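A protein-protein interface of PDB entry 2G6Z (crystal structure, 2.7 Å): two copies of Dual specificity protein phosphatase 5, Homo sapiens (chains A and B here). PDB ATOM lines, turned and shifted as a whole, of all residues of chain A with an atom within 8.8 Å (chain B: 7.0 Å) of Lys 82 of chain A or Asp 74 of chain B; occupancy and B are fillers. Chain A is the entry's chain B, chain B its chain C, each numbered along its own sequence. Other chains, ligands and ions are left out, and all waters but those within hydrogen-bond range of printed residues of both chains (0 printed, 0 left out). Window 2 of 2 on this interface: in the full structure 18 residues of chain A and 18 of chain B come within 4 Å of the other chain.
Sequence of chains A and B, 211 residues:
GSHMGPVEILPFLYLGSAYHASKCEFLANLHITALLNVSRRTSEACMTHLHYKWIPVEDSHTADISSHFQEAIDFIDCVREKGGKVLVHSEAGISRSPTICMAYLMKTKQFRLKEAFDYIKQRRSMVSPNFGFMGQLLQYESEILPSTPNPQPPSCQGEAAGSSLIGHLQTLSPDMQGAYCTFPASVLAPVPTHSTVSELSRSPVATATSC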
ATOM      1  N   PHE A  12     -14.182   6.855  21.329  1.00  0.00           N
ATOM      2  CA  PHE A  12     -15.120   5.784  21.665  1.00  0.00           C
ATOM      3  C   PHE A  12     -14.510   4.709  22.545  1.00  0.00           C
ATOM      4  O   PHE A  12     -15.169   3.708  22.820  1.00  0.00           O
ATOM      5  CB  PHE A  12     -15.583   5.110  20.394  1.00  0.00           C
ATOM      6  CG  PHE A  12     -14.449   4.614  19.558  1.00  0.00           C
ATOM      7  CD1 PHE A  12     -13.753   5.482  18.731  1.00  0.00           C
ATOM      8  CD2 PHE A  12     -14.032   3.295  19.645  1.00  0.00           C
ATOM      9  CE1 PHE A  12     -12.659   5.044  18.003  1.00  0.00           C
ATOM     10  CE2 PHE A  12     -12.935   2.855  18.918  1.00  0.00           C
ATOM     11  CZ  PHE A  12     -12.250   3.737  18.097  1.00  0.00           C
ATOM     12  N   THR A  33     -21.511   3.534  26.812  1.00  0.00           N
ATOM     13  CA  THR A  33     -22.589   2.635  26.412  1.00  0.00           C
ATOM     14  C   THR A  33     -22.270   1.158  26.556  1.00  0.00           C
ATOM     15  O   THR A  33     -23.178   0.327  26.571  1.00  0.00           O
ATOM     16  CB  THR A  33     -23.046   2.886  24.951  1.00  0.00           C
ATOM     17  OG1 THR A  33     -21.985   2.571  24.044  1.00  0.00           O
ATOM     18  CG2 THR A  33     -23.452   4.324  24.761  1.00  0.00           C
ATOM     19  N   ALA A  34     -20.995   0.815  26.672  1.00  0.00           N
ATOM     20  CA  ALA A  34     -20.633  -0.592  26.797  1.00  0.00           C
ATOM     21  C   ALA A  34     -19.440  -0.792  27.698  1.00  0.00           C
ATOM     22  O   ALA A  34     -18.664   0.134  27.947  1.00  0.00           O
ATOM     23  CB  ALA A  34     -20.347  -1.191  25.414  1.00  0.00           C
ATOM     24  N   HIS A  51     -24.163  -2.521  26.823  1.00  0.00           N
ATOM     25  CA  HIS A  51     -23.600  -3.631  26.061  1.00  0.00           C
ATOM     26  C   HIS A  51     -22.415  -4.099  26.919  1.00  0.00           C
ATOM     27  O   HIS A  51     -21.501  -3.329  27.210  1.00  0.00           O
ATOM     28  CB  HIS A  51     -23.110  -3.155  24.687  1.00  0.00           C
ATOM     29  CG  HIS A  51     -24.208  -2.704  23.770  1.00  0.00           C
ATOM     30  ND1 HIS A  51     -25.034  -3.584  23.105  1.00  0.00           N
ATOM     31  CD2 HIS A  51     -24.628  -1.463  23.424  1.00  0.00           C
ATOM     32  CE1 HIS A  51     -25.916  -2.906  22.389  1.00  0.00           C
ATOM     33  NE2 HIS A  51     -25.691  -1.615  22.566  1.00  0.00           N
ATOM     34  N   PHE A  75     -15.396  -6.337  19.215  1.00  0.00           N
ATOM     35  CA  PHE A  75     -16.356  -5.810  20.156  1.00  0.00           C
ATOM     36  C   PHE A  75     -16.241  -4.319  20.214  1.00  0.00           C
ATOM     37  O   PHE A  75     -17.249  -3.626  20.162  1.00  0.00           O
ATOM     38  CB  PHE A  75     -16.150  -6.383  21.557  1.00  0.00           C
ATOM     39  CG  PHE A  75     -17.212  -5.965  22.534  1.00  0.00           C
ATOM     40  CD1 PHE A  75     -18.496  -6.478  22.442  1.00  0.00           C
ATOM     41  CD2 PHE A  75     -16.937  -5.026  23.526  1.00  0.00           C
ATOM     42  CE1 PHE A  75     -19.499  -6.059  23.329  1.00  0.00           C
ATOM     43  CE2 PHE A  75     -17.931  -4.601  24.415  1.00  0.00           C
ATOM     44  CZ  PHE A  75     -19.212  -5.119  24.315  1.00  0.00           C
ATOM     45  N   ILE A  76     -15.019  -3.815  20.331  1.00  0.00           N
ATOM     46  CA  ILE A  76     -14.819  -2.368  20.391  1.00  0.00           C
ATOM     47  C   ILE A  76     -15.232  -1.707  19.076  1.00  0.00           C
ATOM     48  O   ILE A  76     -15.759  -0.596  19.087  1.00  0.00           O
ATOM     49  CB  ILE A  76     -13.359  -2.019  20.705  1.00  0.00           C
ATOM     50  CG1 ILE A  76     -12.985  -2.604  22.059  1.00  0.00           C
ATOM     51  CG2 ILE A  76     -13.168  -0.516  20.758  1.00  0.00           C
ATOM     52  CD1 ILE A  76     -11.493  -2.475  22.370  1.00  0.00           C
ATOM     53  N   ASP A  77     -14.993  -2.381  17.951  1.00  0.00           N
ATOM     54  CA  ASP A  77     -15.390  -1.817  16.667  1.00  0.00           C
ATOM     55  C   ASP A  77     -16.915  -1.703  16.601  1.00  0.00           C
ATOM     56  O   ASP A  77     -17.450  -0.807  15.947  1.00  0.00           O
ATOM     57  CB  ASP A  77     -14.904  -2.670  15.482  1.00  0.00           C
ATOM     58  CG  ASP A  77     -13.444  -2.389  15.095  1.00  0.00           C
ATOM     59  OD1 ASP A  77     -12.930  -1.282  15.386  1.00  0.00           O
ATOM     60  OD2 ASP A  77     -12.813  -3.281  14.473  1.00  0.00           O
ATOM     61  N   CYS A  78     -17.609  -2.607  17.281  1.00  0.00           N
ATOM     62  CA  CYS A  78     -19.060  -2.596  17.269  1.00  0.00           C
ATOM     63  C   CYS A  78     -19.555  -1.317  17.930  1.00  0.00           C
ATOM     64  O   CYS A  78     -20.358  -0.573  17.359  1.00  0.00           O
ATOM     65  CB  CYS A  78     -19.607  -3.824  17.999  1.00  0.00           C
ATOM     66  SG  CYS A  78     -21.369  -4.158  17.688  1.00  0.00           S
ATOM     67  N   VAL A  79     -19.074  -1.058  19.137  1.00  0.00           N
ATOM     68  CA  VAL A  79     -19.458   0.146  19.847  1.00  0.00           C
ATOM     69  C   VAL A  79     -19.100   1.351  18.965  1.00  0.00           C
ATOM     70  O   VAL A  79     -19.847   2.336  18.887  1.00  0.00           O
ATOM     71  CB  VAL A  79     -18.706   0.223  21.186  1.00  0.00           C
ATOM     72  CG1 VAL A  79     -19.162   1.437  22.004  1.00  0.00           C
ATOM     73  CG2 VAL A  79     -18.943  -1.055  21.951  1.00  0.00           C
ATOM     74  N   ARG A  80     -17.954   1.255  18.299  1.00  0.00           N
ATOM     75  CA  ARG A  80     -17.490   2.311  17.407  1.00  0.00           C
ATOM     76  C   ARG A  80     -18.566   2.568  16.350  1.00  0.00           C
ATOM     77  O   ARG A  80     -19.058   3.691  16.215  1.00  0.00           O
ATOM     78  CB  ARG A  80     -16.192   1.891  16.713  1.00  0.00           C
ATOM     79  CG  ARG A  80     -15.413   3.031  16.085  1.00  0.00           C
ATOM     80  CD  ARG A  80     -14.600   2.546  14.899  1.00  0.00           C
ATOM     81  NE  ARG A  80     -13.444   3.404  14.656  1.00  0.00           N
ATOM     82  CZ  ARG A  80     -12.602   3.258  13.635  1.00  0.00           C
ATOM     83  NH1 ARG A  80     -12.801   2.280  12.749  1.00  0.00           N
ATOM     84  NH2 ARG A  80     -11.546   4.070  13.520  1.00  0.00           N
ATOM     85  N   GLU A  81     -18.927   1.529  15.603  1.00  0.00           N
ATOM     86  CA  GLU A  81     -19.953   1.664  14.573  1.00  0.00           C
ATOM     87  C   GLU A  81     -21.267   2.228  15.142  1.00  0.00           C
ATOM     88  O   GLU A  81     -21.880   3.095  14.535  1.00  0.00           O
ATOM     89  CB  GLU A  81     -20.249   0.317  13.926  1.00  0.00           C
ATOM     90  CG  GLU A  81     -19.050  -0.410  13.392  1.00  0.00           C
ATOM     91  CD  GLU A  81     -19.420  -1.783  12.865  1.00  0.00           C
ATOM     92  OE1 GLU A  81     -20.192  -1.859  11.880  1.00  0.00           O
ATOM     93  OE2 GLU A  81     -18.951  -2.787  13.442  1.00  0.00           O
ATOM     94  N   LYS A  82     -21.705   1.736  16.299  1.00  0.00           N
ATOM     95  CA  LYS A  82     -22.950   2.221  16.886  1.00  0.00           C
ATOM     96  C   LYS A  82     -22.791   3.604  17.523  1.00  0.00           C
ATOM     97  O   LYS A  82     -23.693   4.082  18.209  1.00  0.00           O
ATOM     98  CB  LYS A  82     -23.485   1.226  17.928  1.00  0.00           C
ATOM     99  CG  LYS A  82     -23.703  -0.202  17.401  1.00  0.00           C
ATOM    100  CD  LYS A  82     -24.733  -0.995  18.231  1.00  0.00           C
ATOM    101  CE  LYS A  82     -26.166  -0.444  18.007  1.00  0.00           C
ATOM    102  NZ  LYS A  82     -27.283  -1.239  18.627  1.00  0.00           N
ATOM    103  N   GLY A  83     -21.643   4.241  17.299  1.00  0.00           N
ATOM    104  CA  GLY A  83     -21.391   5.567  17.856  1.00  0.00           C
ATOM    105  C   GLY A  83     -21.335   5.677  19.374  1.00  0.00           C
ATOM    106  O   GLY A  83     -21.521   6.761  19.924  1.00  0.00           O
ATOM    107  N   GLY A  84     -21.061   4.569  20.060  1.00  0.00           N
ATOM    108  CA  GLY A  84     -21.009   4.599  21.513  1.00  0.00           C
ATOM    109  C   GLY A  84     -19.617   4.749  22.098  1.00  0.00           C
ATOM    110  O   GLY A  84     -18.719   5.312  21.470  1.00  0.00           O
ATOM    111  N   LYS A  85     -19.438   4.240  23.312  1.00  0.00           N
ATOM    112  CA  LYS A  85     -18.151   4.313  24.000  1.00  0.00           C
ATOM    113  C   LYS A  85     -17.944   3.098  24.906  1.00  0.00           C
ATOM    114  O   LYS A  85     -18.791   2.795  25.757  1.00  0.00           O
ATOM    115  CB  LYS A  85     -18.087   5.592  24.843  1.00  0.00           C
ATOM    116  CG  LYS A  85     -18.086   6.888  24.049  1.00  0.00           C
ATOM    117  CD  LYS A  85     -18.090   8.096  24.987  1.00  0.00           C
ATOM    118  CE  LYS A  85     -18.134   9.419  24.235  1.00  0.00           C
ATOM    119  NZ  LYS A  85     -18.493  10.504  25.184  1.00  0.00           N
ATOM    120  N   HIS B  68     -38.801   0.573  27.007  1.00  0.00           N
ATOM    121  CA  HIS B  68     -37.509  -0.056  26.808  1.00  0.00           C
ATOM    122  C   HIS B  68     -37.520  -0.894  25.547  1.00  0.00           C
ATOM    123  O   HIS B  68     -36.542  -1.546  25.212  1.00  0.00           O
ATOM    124  CB  HIS B  68     -37.168  -0.903  28.019  1.00  0.00           C
ATOM    125  CG  HIS B  68     -36.913  -0.093  29.247  1.00  0.00           C
ATOM    126  ND1 HIS B  68     -37.407  -0.438  30.486  1.00  0.00           N
ATOM    127  CD2 HIS B  68     -36.190   1.037  29.430  1.00  0.00           C
ATOM    128  CE1 HIS B  68     -36.996   0.440  31.382  1.00  0.00           C
ATOM    129  NE2 HIS B  68     -36.255   1.346  30.767  1.00  0.00           N
ATOM    130  N   PHE B  69     -38.631  -0.848  24.833  1.00  0.00           N
ATOM    131  CA  PHE B  69     -38.754  -1.612  23.613  1.00  0.00           C
ATOM    132  C   PHE B  69     -37.636  -1.249  22.658  1.00  0.00           C
ATOM    133  O   PHE B  69     -36.952  -2.129  22.143  1.00  0.00           O
ATOM    134  CB  PHE B  69     -40.121  -1.366  22.963  1.00  0.00           C
ATOM    135  CG  PHE B  69     -41.241  -2.159  23.586  1.00  0.00           C
ATOM    136  CD1 PHE B  69     -41.070  -2.782  24.823  1.00  0.00           C
ATOM    137  CD2 PHE B  69     -42.471  -2.291  22.932  1.00  0.00           C
ATOM    138  CE1 PHE B  69     -42.103  -3.529  25.401  1.00  0.00           C
ATOM    139  CE2 PHE B  69     -43.511  -3.032  23.501  1.00  0.00           C
ATOM    140  CZ  PHE B  69     -43.326  -3.654  24.740  1.00  0.00           C
ATOM    141  N   GLN B  70     -37.428   0.043  22.439  1.00  0.00           N
ATOM    142  CA  GLN B  70     -36.387   0.475  21.512  1.00  0.00           C
ATOM    143  C   GLN B  70     -34.987  -0.051  21.848  1.00  0.00           C
ATOM    144  O   GLN B  70     -34.323  -0.612  20.973  1.00  0.00           O
ATOM    145  CB  GLN B  70     -36.361   2.005  21.405  1.00  0.00           C
ATOM    146  CG  GLN B  70     -35.806   2.526  20.073  1.00  0.00           C
ATOM    147  CD  GLN B  70     -36.387   1.804  18.859  1.00  0.00           C
ATOM    148  OE1 GLN B  70     -35.822   0.822  18.372  1.00  0.00           O
ATOM    149  NE2 GLN B  70     -37.524   2.280  18.377  1.00  0.00           N
ATOM    150  N   GLU B  71     -34.538   0.118  23.093  1.00  0.00           N
ATOM    151  CA  GLU B  71     -33.212  -0.370  23.464  1.00  0.00           C
ATOM    152  C   GLU B  71     -33.114  -1.858  23.119  1.00  0.00           C
ATOM    153  O   GLU B  71     -32.217  -2.280  22.380  1.00  0.00           O
ATOM    154  CB  GLU B  71     -32.947  -0.169  24.953  1.00  0.00           C
ATOM    155  CG  GLU B  71     -31.490  -0.388  25.355  1.00  0.00           C
ATOM    156  CD  GLU B  71     -31.260  -0.288  26.858  1.00  0.00           C
ATOM    157  OE1 GLU B  71     -30.100  -0.493  27.289  1.00  0.00           O
ATOM    158  OE2 GLU B  71     -32.226  -0.008  27.612  1.00  0.00           O
ATOM    159  N   ALA B  72     -34.056  -2.641  23.638  1.00  0.00           N
ATOM    160  CA  ALA B  72     -34.105  -4.077  23.386  1.00  0.00           C
ATOM    161  C   ALA B  72     -34.108  -4.425  21.887  1.00  0.00           C
ATOM    162  O   ALA B  72     -33.377  -5.301  21.439  1.00  0.00           O
ATOM    163  CB  ALA B  72     -35.334  -4.664  24.056  1.00  0.00           C
ATOM    164  N   ILE B  73     -34.940  -3.755  21.112  1.00  0.00           N
ATOM    165  CA  ILE B  73     -34.980  -4.022  19.690  1.00  0.00           C
ATOM    166  C   ILE B  73     -33.639  -3.676  19.033  1.00  0.00           C
ATOM    167  O   ILE B  73     -33.180  -4.394  18.139  1.00  0.00           O
ATOM    168  CB  ILE B  73     -36.122  -3.224  19.005  1.00  0.00           C
ATOM    169  CG1 ILE B  73     -37.462  -3.851  19.383  1.00  0.00           C
ATOM    170  CG2 ILE B  73     -35.943  -3.211  17.484  1.00  0.00           C
ATOM    171  CD1 ILE B  73     -38.673  -3.121  18.832  1.00  0.00           C
ATOM    172  N   ASP B  74     -32.999  -2.593  19.467  1.00  0.00           N
ATOM    173  CA  ASP B  74     -31.719  -2.232  18.861  1.00  0.00           C
ATOM    174  C   ASP B  74     -30.698  -3.301  19.158  1.00  0.00           C
ATOM    175  O   ASP B  74     -29.931  -3.710  18.281  1.00  0.00           O
ATOM    176  CB  ASP B  74     -31.210  -0.876  19.358  1.00  0.00           C
ATOM    177  CG  ASP B  74     -32.040   0.284  18.824  1.00  0.00           C
ATOM    178  OD1 ASP B  74     -32.506   0.185  17.660  1.00  0.00           O
ATOM    179  OD2 ASP B  74     -32.224   1.287  19.560  1.00  0.00           O
ATOM    180  N   PHE B  75     -30.704  -3.767  20.397  1.00  0.00           N
ATOM    181  CA  PHE B  75     -29.775  -4.802  20.792  1.00  0.00           C
ATOM    182  C   PHE B  75     -29.967  -6.017  19.899  1.00  0.00           C
ATOM    183  O   PHE B  75     -29.009  -6.533  19.337  1.00  0.00           O
ATOM    184  CB  PHE B  75     -29.998  -5.209  22.249  1.00  0.00           C
ATOM    185  CG  PHE B  75     -28.951  -6.157  22.775  1.00  0.00           C
ATOM    186  CD1 PHE B  75     -27.652  -5.717  23.011  1.00  0.00           C
ATOM    187  CD2 PHE B  75     -29.254  -7.498  23.007  1.00  0.00           C
ATOM    188  CE1 PHE B  75     -26.668  -6.602  23.475  1.00  0.00           C
ATOM    189  CE2 PHE B  75     -28.283  -8.388  23.466  1.00  0.00           C
ATOM    190  CZ  PHE B  75     -26.988  -7.943  23.703  1.00  0.00           C
ATOM    191  N   ILE B  76     -31.207  -6.472  19.762  1.00  0.00           N
ATOM    192  CA  ILE B  76     -31.474  -7.651  18.955  1.00  0.00           C
ATOM    193  C   ILE B  76     -31.050  -7.432  17.521  1.00  0.00           C
ATOM    194  O   ILE B  76     -30.504  -8.343  16.889  1.00  0.00           O
ATOM    195  CB  ILE B  76     -32.975  -8.065  19.014  1.00  0.00           C
ATOM    196  CG1 ILE B  76     -33.326  -8.490  20.441  1.00  0.00           C
ATOM    197  CG2 ILE B  76     -33.249  -9.248  18.071  1.00  0.00           C
ATOM    198  CD1 ILE B  76     -34.812  -8.727  20.666  1.00  0.00           C
ATOM    199  N   ASP B  77     -31.291  -6.231  17.002  1.00  0.00           N
ATOM    200  CA  ASP B  77     -30.903  -5.947  15.630  1.00  0.00           C
ATOM    201  C   ASP B  77     -29.387  -5.894  15.511  1.00  0.00           C
ATOM    202  O   ASP B  77     -28.833  -6.207  14.458  1.00  0.00           O
ATOM    203  CB  ASP B  77     -31.526  -4.637  15.129  1.00  0.00           C
ATOM    204  CG  ASP B  77     -32.964  -4.823  14.601  1.00  0.00           C
ATOM    205  OD1 ASP B  77     -33.221  -5.796  13.855  1.00  0.00           O
ATOM    206  OD2 ASP B  77     -33.836  -3.984  14.919  1.00  0.00           O
ATOM    207  N   CYS B  78     -28.712  -5.511  16.592  1.00  0.00           N
ATOM    208  CA  CYS B  78     -27.261  -5.453  16.566  1.00  0.00           C
ATOM    209  C   CYS B  78     -26.772  -6.878  16.328  1.00  0.00           C
ATOM    210  O   CYS B  78     -26.027  -7.144  15.383  1.00  0.00           O
ATOM    211  CB  CYS B  78     -26.715  -4.902  17.887  1.00  0.00           C
ATOM    212  SG  CYS B  78     -24.914  -4.525  17.895  1.00  0.00           S
ATOM    213  N   VAL B  79     -27.211  -7.798  17.178  1.00  0.00           N
ATOM    214  CA  VAL B  79     -26.836  -9.200  17.049  1.00  0.00           C
ATOM    215  C   VAL B  79     -27.160  -9.703  15.634  1.00  0.00           C
ATOM    216  O   VAL B  79     -26.359 -10.395  15.009  1.00  0.00           O
ATOM    217  CB  VAL B  79     -27.571 -10.058  18.125  1.00  0.00           C
ATOM    218  CG1 VAL B  79     -27.359 -11.561  17.881  1.00  0.00           C
ATOM    219  CG2 VAL B  79     -27.039  -9.690  19.499  1.00  0.00           C
ATOM    220  N   ARG B  80     -28.333  -9.336  15.131  1.00  0.00           N
ATOM    221  CA  ARG B  80     -28.759  -9.740  13.791  1.00  0.00           C
ATOM    222  C   ARG B  80     -27.697  -9.353  12.753  1.00  0.00           C
ATOM    223  O   ARG B  80     -27.262 -10.191  11.949  1.00  0.00           O
ATOM    224  CB  ARG B  80     -30.095  -9.065  13.436  1.00  0.00           C
ATOM    225  CG  ARG B  80     -30.775  -9.642  12.207  1.00  0.00           C
ATOM    226  CD  ARG B  80     -31.859  -8.720  11.667  1.00  0.00           C
ATOM    227  NE  ARG B  80     -32.615  -9.373  10.600  1.00  0.00           N
ATOM    228  CZ  ARG B  80     -33.684  -8.854  10.001  1.00  0.00           C
ATOM    229  NH1 ARG B  80     -34.137  -7.657  10.358  1.00  0.00           N
ATOM    230  NH2 ARG B  80     -34.313  -9.548   9.059  1.00  0.00           N
ATOM    231  N   GLU B  81     -27.297  -8.082  12.774  1.00  0.00           N
ATOM    232  CA  GLU B  81     -26.290  -7.560  11.855  1.00  0.00           C
ATOM    233  C   GLU B  81     -24.975  -8.328  11.962  1.00  0.00           C
ATOM    234  O   GLU B  81     -24.413  -8.751  10.949  1.00  0.00           O
ATOM    235  CB  GLU B  81     -26.013  -6.087  12.142  1.00  0.00           C
ATOM    236  CG  GLU B  81     -27.215  -5.185  12.038  1.00  0.00           C
ATOM    237  CD  GLU B  81     -26.832  -3.721  12.165  1.00  0.00           C
ATOM    238  OE1 GLU B  81     -26.063  -3.240  11.302  1.00  0.00           O
ATOM    239  OE2 GLU B  81     -27.291  -3.053  13.122  1.00  0.00           O
ATOM    240  N   TYR B 104     -40.637  -6.931  19.154  1.00  0.00           N
ATOM    241  CA  TYR B 104     -39.699  -7.053  18.046  1.00  0.00           C
ATOM    242  C   TYR B 104     -40.394  -7.434  16.746  1.00  0.00           C
ATOM    243  O   TYR B 104     -40.180  -6.792  15.717  1.00  0.00           O
ATOM    244  CB  TYR B 104     -38.594  -8.075  18.353  1.00  0.00           C
ATOM    245  CG  TYR B 104     -37.474  -8.076  17.323  1.00  0.00           C
ATOM    246  CD1 TYR B 104     -36.467  -7.092  17.343  1.00  0.00           C
ATOM    247  CD2 TYR B 104     -37.469  -8.998  16.275  1.00  0.00           C
ATOM    248  CE1 TYR B 104     -35.491  -7.028  16.336  1.00  0.00           C
ATOM    249  CE2 TYR B 104     -36.504  -8.947  15.260  1.00  0.00           C
ATOM    250  CZ  TYR B 104     -35.519  -7.959  15.293  1.00  0.00           C
ATOM    251  OH  TYR B 104     -34.585  -7.909  14.277  1.00  0.00           O
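Of the 15 printed residues of chain A, 3 touch a printed residue of chain B.
Printed residues of chain A that touch a printed residue of chain B: His 51, Cys 78 and Lys 82.
Hydrophobic or aromatic side chains of chain A that line the printed part of chain B: His 51.
Of the 15 printed residues of chain B, 3 touch a printed residue of chain A.
Printed residues of chain B that touch a printed residue of chain A: Asp 74, Phe 75 and Cys 78.
Hydrophobic or aromatic side chains of chain B within 4 Å of the printed part of chain A: Phe 75.
Among the printed residues, 4 pairs touch across the chains.
Among the printed residues, pairs that only touch across the chains: His 51 of chain A with Phe 75 of chain B, Lys 82 of chain A with Asp 74 of chain B and Lys 82 of chain A with Cys 78 of chain B.
Phe 12 of chain A touches none of the printed residues of chain B.
Of the printed residues of chain B, His 51 of chain A touches Phe 75.
Of the printed residues of chain B, Cys 78 of chain A touches Cys 78.
Lys 82 of chain A touches just these residues of chain B: Asp 74 and Cys 78.
Asp 74 of chain B touches just one residue of chain A: Lys 82.
Of the printed residues of chain A, Phe 75 of chain B touches His 51.
Of the printed residues of chain A, Cys 78 of chain B touches Cys 78 and Lys 82.
The nearest residue of chain B that does not touch Lys 82 of chain A is Phe 75 of chain B (4.6 Å).
Cys 78 of chain B touches its own counterpart, Cys 78 of chain A.
O of Thr 33 of chain A sits at hydrogen-bond distance from N of His 51 of chain A, 3.0 Å away.
OE1 of Gln 70 of chain B sits close to OD1 of Asp 74 of chain B (3.5 Å).
The side-chain sulfur (SG) of Cys 78 of chain A is in hydrogen-bond range of the side-chain sulfur (SG) of Cys 78 of chain B.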
